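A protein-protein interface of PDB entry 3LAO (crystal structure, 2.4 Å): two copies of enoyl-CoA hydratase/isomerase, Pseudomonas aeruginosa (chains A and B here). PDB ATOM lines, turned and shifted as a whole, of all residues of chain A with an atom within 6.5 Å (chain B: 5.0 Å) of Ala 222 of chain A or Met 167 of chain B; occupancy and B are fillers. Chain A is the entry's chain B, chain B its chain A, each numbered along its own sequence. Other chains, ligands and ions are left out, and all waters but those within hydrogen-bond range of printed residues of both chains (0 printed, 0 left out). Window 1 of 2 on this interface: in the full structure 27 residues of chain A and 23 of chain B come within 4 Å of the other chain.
Among the printed residues, pairs that only touch across the chains: Ala 127 of chain A with Trp 163 of chain B (3.3 Å), Asp 128 of chain A with Met 167 of chain B (3.5 Å), Ile 129 of chain A with Thr 164 of chain B (3.4 Å), Ile 129 of chain A with Arg 168 of chain B (3.6 Å), Ile 207 of chain A with Leu 171 of chain B (3.8 Å), Ile 207 of chain A with Thr 172 of chain B (3.98 Å), Ala 218 of chain A with Ile 170 of chain B (3.8 Å), Ala 218 of chain A with Leu 171 of chain B (3.9 Å), Ser 221 of chain A with Val 155 of chain B (3.4 Å), Ala 222 of chain A with Val 155 of chain B (3.7 Å), Ala 222 of chain A with Trp 163 of chain B (3.3 Å), Ala 222 of chain A with Met 167 of chain B (3.4 Å), Phe 223 of chain A with Trp 163 of chain B (3.6 Å), Gln 224 of chain A with Val 155 of chain B (3.7 Å) and Arg 226 of chain A with Trp 163 of chain B (3.5 Å).
Of the 14 printed residues of chain A, 10 touch a printed residue of chain B. Hydrophobic or aromatic side chains of chain A within 4 Å of the printed part of chain B: Ile 129, Ile 207, Ala 218, Ala 222 and Phe 223. Of the 13 printed residues of chain B, 8 touch a printed residue of chain A. Among the printed residues, 17 pairs touch across the chains.
The side-chain hydroxyl (OG1) of Thr 172 of chain B lies within hydrogen-bond range of the backbone carbonyl oxygen (O) of Arg 168 of chain B (2.6 Å). The side-chain hydroxyl (OG) of Ser 221 of chain A is in hydrogen-bond range of the backbone carbonyl oxygen (O) of Ala 217 of chain A, 3.3 Å away. The side-chain amide oxygen (OE1) of Gln 224 of chain A sits close to the backbone carbonyl oxygen (O) of Gln 220 of chain A (3.1 Å).
Of chain B, only Val 155, Trp 163 and Met 167 come within 4 Å of Ala 222 of chain A. Of chain A, only Asp 128 and Ala 222 come within 4 Å of Met 167 of chain B. Printed residues of chain A within 4 Å of Trp 163 of chain B: Ala 127 (3.3 Å), Asp 128 (2.8 Å), Ala 222 (3.3 Å), Phe 223 (3.6 Å) and Arg 226 (3.5 Å). Printed residues of chain A within 4 Å of Val 155 of chain B: Ser 221 (3.4 Å), Ala 222 (3.7 Å) and Gln 224 (3.7 Å). Of the printed residues of chain B, Arg 226 of chain A touches Trp 163. Printed residues of chain A within 4 Å of Arg 168 of chain B: Ile 129 (3.6 Å). Of the printed residues of chain A, Thr 172 of chain B touches Ile 207. Leu 219 of chain A touches none of the printed residues of chain B. Ala 166 of chain B touches none of the printed residues of chain A.
No position is printed for both chains. Of the 17 pairs that touch across the chains among the printed residues, none has its exchanged pair printed and touching as well.
The indole nitrogen (NE1) of Trp 163 of chain B sits at hydrogen-bond distance from the side-chain carboxylate (OD1) of Asp 128 of chain A, 2.8 Å away. The side-chain hydroxyl of Thr 164 of chain B is in hydrogen-bond range of the backbone carbonyl oxygen of Asp 128 of chain A (2.9 Å).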
ATOM      1  N   ALA A 127      28.399  13.798 -17.051  1.00  0.00           N
ATOM      2  CA  ALA A 127      27.182  13.185 -17.552  1.00  0.00           C
ATOM      3  C   ALA A 127      26.772  11.965 -16.695  1.00  0.00           C
ATOM      4  O   ALA A 127      27.519  11.512 -15.841  1.00  0.00           O
ATOM      5  CB  ALA A 127      27.392  12.768 -18.978  1.00  0.00           C
ATOM      6  N   ASP A 128      25.584  11.435 -16.938  1.00  0.00           N
ATOM      7  CA  ASP A 128      25.104  10.273 -16.195  1.00  0.00           C
ATOM      8  C   ASP A 128      25.344   8.944 -16.877  1.00  0.00           C
ATOM      9  O   ASP A 128      25.395   7.921 -16.238  1.00  0.00           O
ATOM     10  CB  ASP A 128      23.639  10.476 -15.966  1.00  0.00           C
ATOM     11  CG  ASP A 128      23.379  11.791 -15.308  1.00  0.00           C
ATOM     12  OD1 ASP A 128      24.129  12.100 -14.362  1.00  0.00           O
ATOM     13  OD2 ASP A 128      22.481  12.530 -15.763  1.00  0.00           O
ATOM     14  N   ILE A 129      25.454   8.973 -18.191  1.00  0.00           N
ATOM     15  CA  ILE A 129      25.778   7.816 -19.005  1.00  0.00           C
ATOM     16  C   ILE A 129      26.724   8.309 -20.079  1.00  0.00           C
ATOM     17  O   ILE A 129      26.485   9.368 -20.726  1.00  0.00           O
ATOM     18  CB  ILE A 129      24.578   7.283 -19.749  1.00  0.00           C
ATOM     19  CG1 ILE A 129      23.410   6.996 -18.784  1.00  0.00           C
ATOM     20  CG2 ILE A 129      25.003   6.087 -20.615  1.00  0.00           C
ATOM     21  CD1 ILE A 129      23.637   5.912 -17.792  1.00  0.00           C
ATOM     22  N   ILE A 207      15.820   6.268 -20.001  1.00  0.00           N
ATOM     23  CA  ILE A 207      15.689   7.215 -18.908  1.00  0.00           C
ATOM     24  C   ILE A 207      14.425   8.030 -19.153  1.00  0.00           C
ATOM     25  O   ILE A 207      13.709   8.416 -18.221  1.00  0.00           O
ATOM     26  CB  ILE A 207      16.919   8.185 -18.861  1.00  0.00           C
ATOM     27  CG1 ILE A 207      18.191   7.466 -18.389  1.00  0.00           C
ATOM     28  CG2 ILE A 207      16.653   9.456 -18.039  1.00  0.00           C
ATOM     29  CD1 ILE A 207      19.503   8.331 -18.611  1.00  0.00           C
ATOM     30  N   ALA A 217      14.187  13.754  -8.701  1.00  0.00           N
ATOM     31  CA  ALA A 217      14.465  13.616  -7.276  1.00  0.00           C
ATOM     32  C   ALA A 217      15.623  12.620  -7.029  1.00  0.00           C
ATOM     33  O   ALA A 217      16.400  12.780  -6.098  1.00  0.00           O
ATOM     34  CB  ALA A 217      13.236  13.177  -6.557  1.00  0.00           C
ATOM     35  N   ALA A 218      15.749  11.610  -7.880  1.00  0.00           N
ATOM     36  CA  ALA A 218      16.918  10.747  -7.816  1.00  0.00           C
ATOM     37  C   ALA A 218      18.222  11.550  -8.009  1.00  0.00           C
ATOM     38  O   ALA A 218      19.154  11.424  -7.165  1.00  0.00           O
ATOM     39  CB  ALA A 218      16.803   9.593  -8.803  1.00  0.00           C
ATOM     40  N   LEU A 219      18.263  12.393  -9.068  1.00  0.00           N
ATOM     41  CA  LEU A 219      19.473  13.174  -9.407  1.00  0.00           C
ATOM     42  C   LEU A 219      19.821  14.093  -8.275  1.00  0.00           C
ATOM     43  O   LEU A 219      20.998  14.220  -7.892  1.00  0.00           O
ATOM     44  CB  LEU A 219      19.320  14.008 -10.674  1.00  0.00           C
ATOM     45  CG  LEU A 219      19.530  13.216 -11.950  1.00  0.00           C
ATOM     46  CD1 LEU A 219      19.039  14.013 -13.121  1.00  0.00           C
ATOM     47  CD2 LEU A 219      20.997  12.807 -12.143  1.00  0.00           C
ATOM     48  N   GLN A 220      18.788  14.736  -7.746  1.00  0.00           N
ATOM     49  CA  GLN A 220      18.959  15.676  -6.637  1.00  0.00           C
ATOM     50  C   GLN A 220      19.521  14.975  -5.390  1.00  0.00           C
ATOM     51  O   GLN A 220      20.428  15.518  -4.751  1.00  0.00           O
ATOM     52  CB  GLN A 220      17.662  16.445  -6.321  1.00  0.00           C
ATOM     53  CG  GLN A 220      17.859  17.650  -5.422  1.00  0.00           C
ATOM     54  CD  GLN A 220      18.645  18.750  -6.130  1.00  0.00           C
ATOM     55  OE1 GLN A 220      18.696  18.801  -7.373  1.00  0.00           O
ATOM     56  NE2 GLN A 220      19.268  19.628  -5.349  1.00  0.00           N
ATOM     57  N   SER A 221      19.054  13.767  -5.056  1.00  0.00           N
ATOM     58  CA  SER A 221      19.726  13.049  -3.941  1.00  0.00           C
ATOM     59  C   SER A 221      21.191  12.715  -4.218  1.00  0.00           C
ATOM     60  O   SER A 221      22.048  12.857  -3.351  1.00  0.00           O
ATOM     61  CB  SER A 221      19.002  11.765  -3.591  1.00  0.00           C
ATOM     62  OG  SER A 221      17.737  12.100  -3.117  1.00  0.00           O
ATOM     63  N   ALA A 222      21.469  12.263  -5.435  1.00  0.00           N
ATOM     64  CA  ALA A 222      22.815  11.813  -5.791  1.00  0.00           C
ATOM     65  C   ALA A 222      23.794  12.983  -5.762  1.00  0.00           C
ATOM     66  O   ALA A 222      24.901  12.870  -5.204  1.00  0.00           O
ATOM     67  CB  ALA A 222      22.800  11.121  -7.161  1.00  0.00           C
ATOM     68  N   PHE A 223      23.338  14.126  -6.282  1.00  0.00           N
ATOM     69  CA  PHE A 223      24.135  15.339  -6.352  1.00  0.00           C
ATOM     70  C   PHE A 223      24.620  15.855  -4.998  1.00  0.00           C
ATOM     71  O   PHE A 223      25.424  16.765  -4.968  1.00  0.00           O
ATOM     72  CB  PHE A 223      23.399  16.452  -7.103  1.00  0.00           C
ATOM     73  CG  PHE A 223      23.415  16.310  -8.623  1.00  0.00           C
ATOM     74  CD1 PHE A 223      24.555  15.924  -9.298  1.00  0.00           C
ATOM     75  CD2 PHE A 223      22.301  16.635  -9.371  1.00  0.00           C
ATOM     76  CE1 PHE A 223      24.566  15.806 -10.688  1.00  0.00           C
ATOM     77  CE2 PHE A 223      22.311  16.527 -10.751  1.00  0.00           C
ATOM     78  CZ  PHE A 223      23.442  16.093 -11.412  1.00  0.00           C
ATOM     79  N   GLN A 224      24.161  15.276  -3.889  1.00  0.00           N
ATOM     80  CA  GLN A 224      24.677  15.640  -2.555  1.00  0.00           C
ATOM     81  C   GLN A 224      26.150  15.303  -2.304  1.00  0.00           C
ATOM     82  O   GLN A 224      26.544  14.129  -2.218  1.00  0.00           O
ATOM     83  CB  GLN A 224      23.842  15.010  -1.454  1.00  0.00           C
ATOM     84  CG  GLN A 224      22.414  15.453  -1.505  1.00  0.00           C
ATOM     85  CD  GLN A 224      22.280  16.933  -1.837  1.00  0.00           C
ATOM     86  OE1 GLN A 224      22.186  17.308  -3.003  1.00  0.00           O
ATOM     87  NE2 GLN A 224      22.273  17.777  -0.808  1.00  0.00           N
ATOM     88  N   GLY A 225      26.963  16.343  -2.172  1.00  0.00           N
ATOM     89  CA  GLY A 225      28.369  16.193  -1.863  1.00  0.00           C
ATOM     90  C   GLY A 225      29.149  15.440  -2.914  1.00  0.00           C
ATOM     91  O   GLY A 225      30.230  14.930  -2.643  1.00  0.00           O
ATOM     92  N   ARG A 226      28.605  15.374  -4.118  1.00  0.00           N
ATOM     93  CA  ARG A 226      29.239  14.641  -5.204  1.00  0.00           C
ATOM     94  C   ARG A 226      30.689  15.076  -5.447  1.00  0.00           C
ATOM     95  O   ARG A 226      31.579  14.245  -5.625  1.00  0.00           O
ATOM     96  CB  ARG A 226      28.416  14.782  -6.482  1.00  0.00           C
ATOM     97  CG  ARG A 226      28.953  14.008  -7.653  1.00  0.00           C
ATOM     98  CD  ARG A 226      28.467  14.594  -8.954  1.00  0.00           C
ATOM     99  NE  ARG A 226      28.859  13.775 -10.090  1.00  0.00           N
ATOM    100  CZ  ARG A 226      28.583  14.073 -11.350  1.00  0.00           C
ATOM    101  NH1 ARG A 226      27.912  15.176 -11.637  1.00  0.00           N
ATOM    102  NH2 ARG A 226      28.978  13.272 -12.323  1.00  0.00           N
ATOM    103  N   THR B 154      19.982   7.185  -2.648  1.00  0.00           N
ATOM    104  CA  THR B 154      20.784   8.221  -2.019  1.00  0.00           C
ATOM    105  C   THR B 154      22.104   8.272  -2.742  1.00  0.00           C
ATOM    106  O   THR B 154      22.213   7.795  -3.849  1.00  0.00           O
ATOM    107  CB  THR B 154      21.036   7.907  -0.514  1.00  0.00           C
ATOM    108  OG1 THR B 154      21.772   6.676  -0.384  1.00  0.00           O
ATOM    109  CG2 THR B 154      19.697   7.832   0.251  1.00  0.00           C
ATOM    110  N   VAL B 155      23.115   8.805  -2.090  1.00  0.00           N
ATOM    111  CA  VAL B 155      24.473   8.839  -2.632  1.00  0.00           C
ATOM    112  C   VAL B 155      25.220   7.525  -2.467  1.00  0.00           C
ATOM    113  O   VAL B 155      26.289   7.346  -3.054  1.00  0.00           O
ATOM    114  CB  VAL B 155      25.307   9.922  -1.951  1.00  0.00           C
ATOM    115  CG1 VAL B 155      26.413  10.378  -2.881  1.00  0.00           C
ATOM    116  CG2 VAL B 155      24.430  11.080  -1.711  1.00  0.00           C
ATOM    117  N   PRO B 158      25.987   5.636  -6.044  1.00  0.00           N
ATOM    118  CA  PRO B 158      27.069   6.285  -6.795  1.00  0.00           C
ATOM    119  C   PRO B 158      28.407   6.140  -6.088  1.00  0.00           C
ATOM    120  O   PRO B 158      29.379   5.890  -6.765  1.00  0.00           O
ATOM    121  CB  PRO B 158      26.692   7.771  -6.770  1.00  0.00           C
ATOM    122  CG  PRO B 158      25.333   7.817  -6.410  1.00  0.00           C
ATOM    123  CD  PRO B 158      24.963   6.597  -5.644  1.00  0.00           C
ATOM    124  N   TRP B 163      29.621   6.984 -10.450  1.00  0.00           N
ATOM    125  CA  TRP B 163      28.476   7.753 -10.894  1.00  0.00           C
ATOM    126  C   TRP B 163      27.723   7.112 -12.048  1.00  0.00           C
ATOM    127  O   TRP B 163      26.528   6.880 -11.939  1.00  0.00           O
ATOM    128  CB  TRP B 163      28.899   9.181 -11.307  1.00  0.00           C
ATOM    129  CG  TRP B 163      27.696  10.053 -11.553  1.00  0.00           C
ATOM    130  CD1 TRP B 163      27.109  10.332 -12.759  1.00  0.00           C
ATOM    131  CD2 TRP B 163      26.921  10.746 -10.565  1.00  0.00           C
ATOM    132  NE1 TRP B 163      26.025  11.170 -12.580  1.00  0.00           N
ATOM    133  CE2 TRP B 163      25.895  11.443 -11.244  1.00  0.00           C
ATOM    134  CE3 TRP B 163      27.009  10.865  -9.172  1.00  0.00           C
ATOM    135  CZ2 TRP B 163      24.952  12.225 -10.575  1.00  0.00           C
ATOM    136  CZ3 TRP B 163      26.067  11.643  -8.497  1.00  0.00           C
ATOM    137  CH2 TRP B 163      25.061  12.325  -9.207  1.00  0.00           C
ATOM    138  N   THR B 164      28.414   6.850 -13.163  1.00  0.00           N
ATOM    139  CA  THR B 164      27.712   6.357 -14.336  1.00  0.00           C
ATOM    140  C   THR B 164      27.076   4.979 -14.154  1.00  0.00           C
ATOM    141  O   THR B 164      25.942   4.805 -14.512  1.00  0.00           O
ATOM    142  CB  THR B 164      28.536   6.405 -15.624  1.00  0.00           C
ATOM    143  OG1 THR B 164      27.656   6.199 -16.731  1.00  0.00           O
ATOM    144  CG2 THR B 164      29.641   5.325 -15.644  1.00  0.00           C
ATOM    145  N   ASP B 165      27.770   3.999 -13.590  1.00  0.00           N
ATOM    146  CA  ASP B 165      27.092   2.708 -13.365  1.00  0.00           C
ATOM    147  C   ASP B 165      25.895   2.842 -12.442  1.00  0.00           C
ATOM    148  O   ASP B 165      24.879   2.197 -12.654  1.00  0.00           O
ATOM    149  CB  ASP B 165      28.042   1.599 -12.886  1.00  0.00           C
ATOM    150  CG  ASP B 165      28.843   1.004 -14.026  1.00  0.00           C
ATOM    151  OD1 ASP B 165      28.437   1.213 -15.197  1.00  0.00           O
ATOM    152  OD2 ASP B 165      29.879   0.347 -13.756  1.00  0.00           O
ATOM    153  N   ALA B 166      26.000   3.690 -11.428  1.00  0.00           N
ATOM    154  CA  ALA B 166      24.855   3.880 -10.564  1.00  0.00           C
ATOM    155  C   ALA B 166      23.691   4.498 -11.347  1.00  0.00           C
ATOM    156  O   ALA B 166      22.571   3.952 -11.286  1.00  0.00           O
ATOM    157  CB  ALA B 166      25.207   4.700  -9.307  1.00  0.00           C
ATOM    158  N   MET B 167      23.939   5.600 -12.078  1.00  0.00           N
ATOM    159  CA  MET B 167      22.850   6.225 -12.825  1.00  0.00           C
ATOM    160  C   MET B 167      22.257   5.254 -13.861  1.00  0.00           C
ATOM    161  O   MET B 167      21.061   5.325 -14.153  1.00  0.00           O
ATOM    162  CB  MET B 167      23.243   7.572 -13.481  1.00  0.00           C
ATOM    163  CG  MET B 167      23.569   8.728 -12.480  1.00  0.00           C
ATOM    164  SD  MET B 167      22.320   8.920 -10.993  1.00  0.00           S
ATOM    165  CE  MET B 167      23.583   8.743  -9.491  1.00  0.00           C
ATOM    166  N   ARG B 168      23.076   4.353 -14.402  1.00  0.00           N
ATOM    167  CA  ARG B 168      22.564   3.423 -15.410  1.00  0.00           C
ATOM    168  C   ARG B 168      21.314   2.714 -14.853  1.00  0.00           C
ATOM    169  O   ARG B 168      20.367   2.425 -15.581  1.00  0.00           O
ATOM    170  CB  ARG B 168      23.636   2.396 -15.810  1.00  0.00           C
ATOM    171  CG  ARG B 168      23.116   0.948 -15.932  1.00  0.00           C
ATOM    172  CD  ARG B 168      22.907   0.636 -17.385  1.00  0.00           C
ATOM    173  NE  ARG B 168      22.247  -0.620 -17.718  1.00  0.00           N
ATOM    174  CZ  ARG B 168      20.935  -0.744 -17.866  1.00  0.00           C
ATOM    175  NH1 ARG B 168      20.431  -1.909 -18.230  1.00  0.00           N
ATOM    176  NH2 ARG B 168      20.119   0.283 -17.624  1.00  0.00           N
ATOM    177  N   TYR B 169      21.317   2.446 -13.551  1.00  0.00           N
ATOM    178  CA  TYR B 169      20.218   1.692 -12.914  1.00  0.00           C
ATOM    179  C   TYR B 169      19.226   2.552 -12.119  1.00  0.00           C
ATOM    180  O   TYR B 169      18.059   2.273 -12.113  1.00  0.00           O
ATOM    181  CB  TYR B 169      20.742   0.543 -12.049  1.00  0.00           C
ATOM    182  CG  TYR B 169      21.434  -0.519 -12.870  1.00  0.00           C
ATOM    183  CD1 TYR B 169      20.701  -1.331 -13.730  1.00  0.00           C
ATOM    184  CD2 TYR B 169      22.826  -0.716 -12.791  1.00  0.00           C
ATOM    185  CE1 TYR B 169      21.317  -2.302 -14.501  1.00  0.00           C
ATOM    186  CE2 TYR B 169      23.476  -1.719 -13.573  1.00  0.00           C
ATOM    187  CZ  TYR B 169      22.705  -2.503 -14.423  1.00  0.00           C
ATOM    188  OH  TYR B 169      23.287  -3.512 -15.207  1.00  0.00           O
ATOM    189  N   ILE B 170      19.704   3.611 -11.488  1.00  0.00           N
ATOM    190  CA  ILE B 170      18.873   4.475 -10.698  1.00  0.00           C
ATOM    191  C   ILE B 170      17.853   5.257 -11.566  1.00  0.00           C
ATOM    192  O   ILE B 170      16.697   5.397 -11.194  1.00  0.00           O
ATOM    193  CB  ILE B 170      19.773   5.407  -9.852  1.00  0.00           C
ATOM    194  CG1 ILE B 170      20.456   4.583  -8.781  1.00  0.00           C
ATOM    195  CG2 ILE B 170      18.982   6.508  -9.195  1.00  0.00           C
ATOM    196  CD1 ILE B 170      21.489   5.336  -8.041  1.00  0.00           C
ATOM    197  N   LEU B 171      18.273   5.734 -12.733  1.00  0.00           N
ATOM    198  CA  LEU B 171      17.386   6.514 -13.600  1.00  0.00           C
ATOM    199  C   LEU B 171      16.541   5.679 -14.576  1.00  0.00           C
ATOM    200  O   LEU B 171      15.657   6.207 -15.197  1.00  0.00           O
ATOM    201  CB  LEU B 171      18.173   7.583 -14.371  1.00  0.00           C
ATOM    202  CG  LEU B 171      19.131   8.401 -13.491  1.00  0.00           C
ATOM    203  CD1 LEU B 171      19.888   9.451 -14.321  1.00  0.00           C
ATOM    204  CD2 LEU B 171      18.373   9.063 -12.376  1.00  0.00           C
ATOM    205  N   THR B 172      16.788   4.380 -14.695  1.00  0.00           N
ATOM    206  CA  THR B 172      16.007   3.530 -15.621  1.00  0.00           C
ATOM    207  C   THR B 172      15.097   2.549 -14.890  1.00  0.00           C
ATOM    208  O   THR B 172      14.104   2.066 -15.444  1.00  0.00           O
ATOM    209  CB  THR B 172      16.942   2.702 -16.526  1.00  0.00           C
ATOM    210  OG1 THR B 172      17.820   1.874 -15.726  1.00  0.00           O
ATOM    211  CG2 THR B 172      17.811   3.644 -17.335  1.00  0.00           C
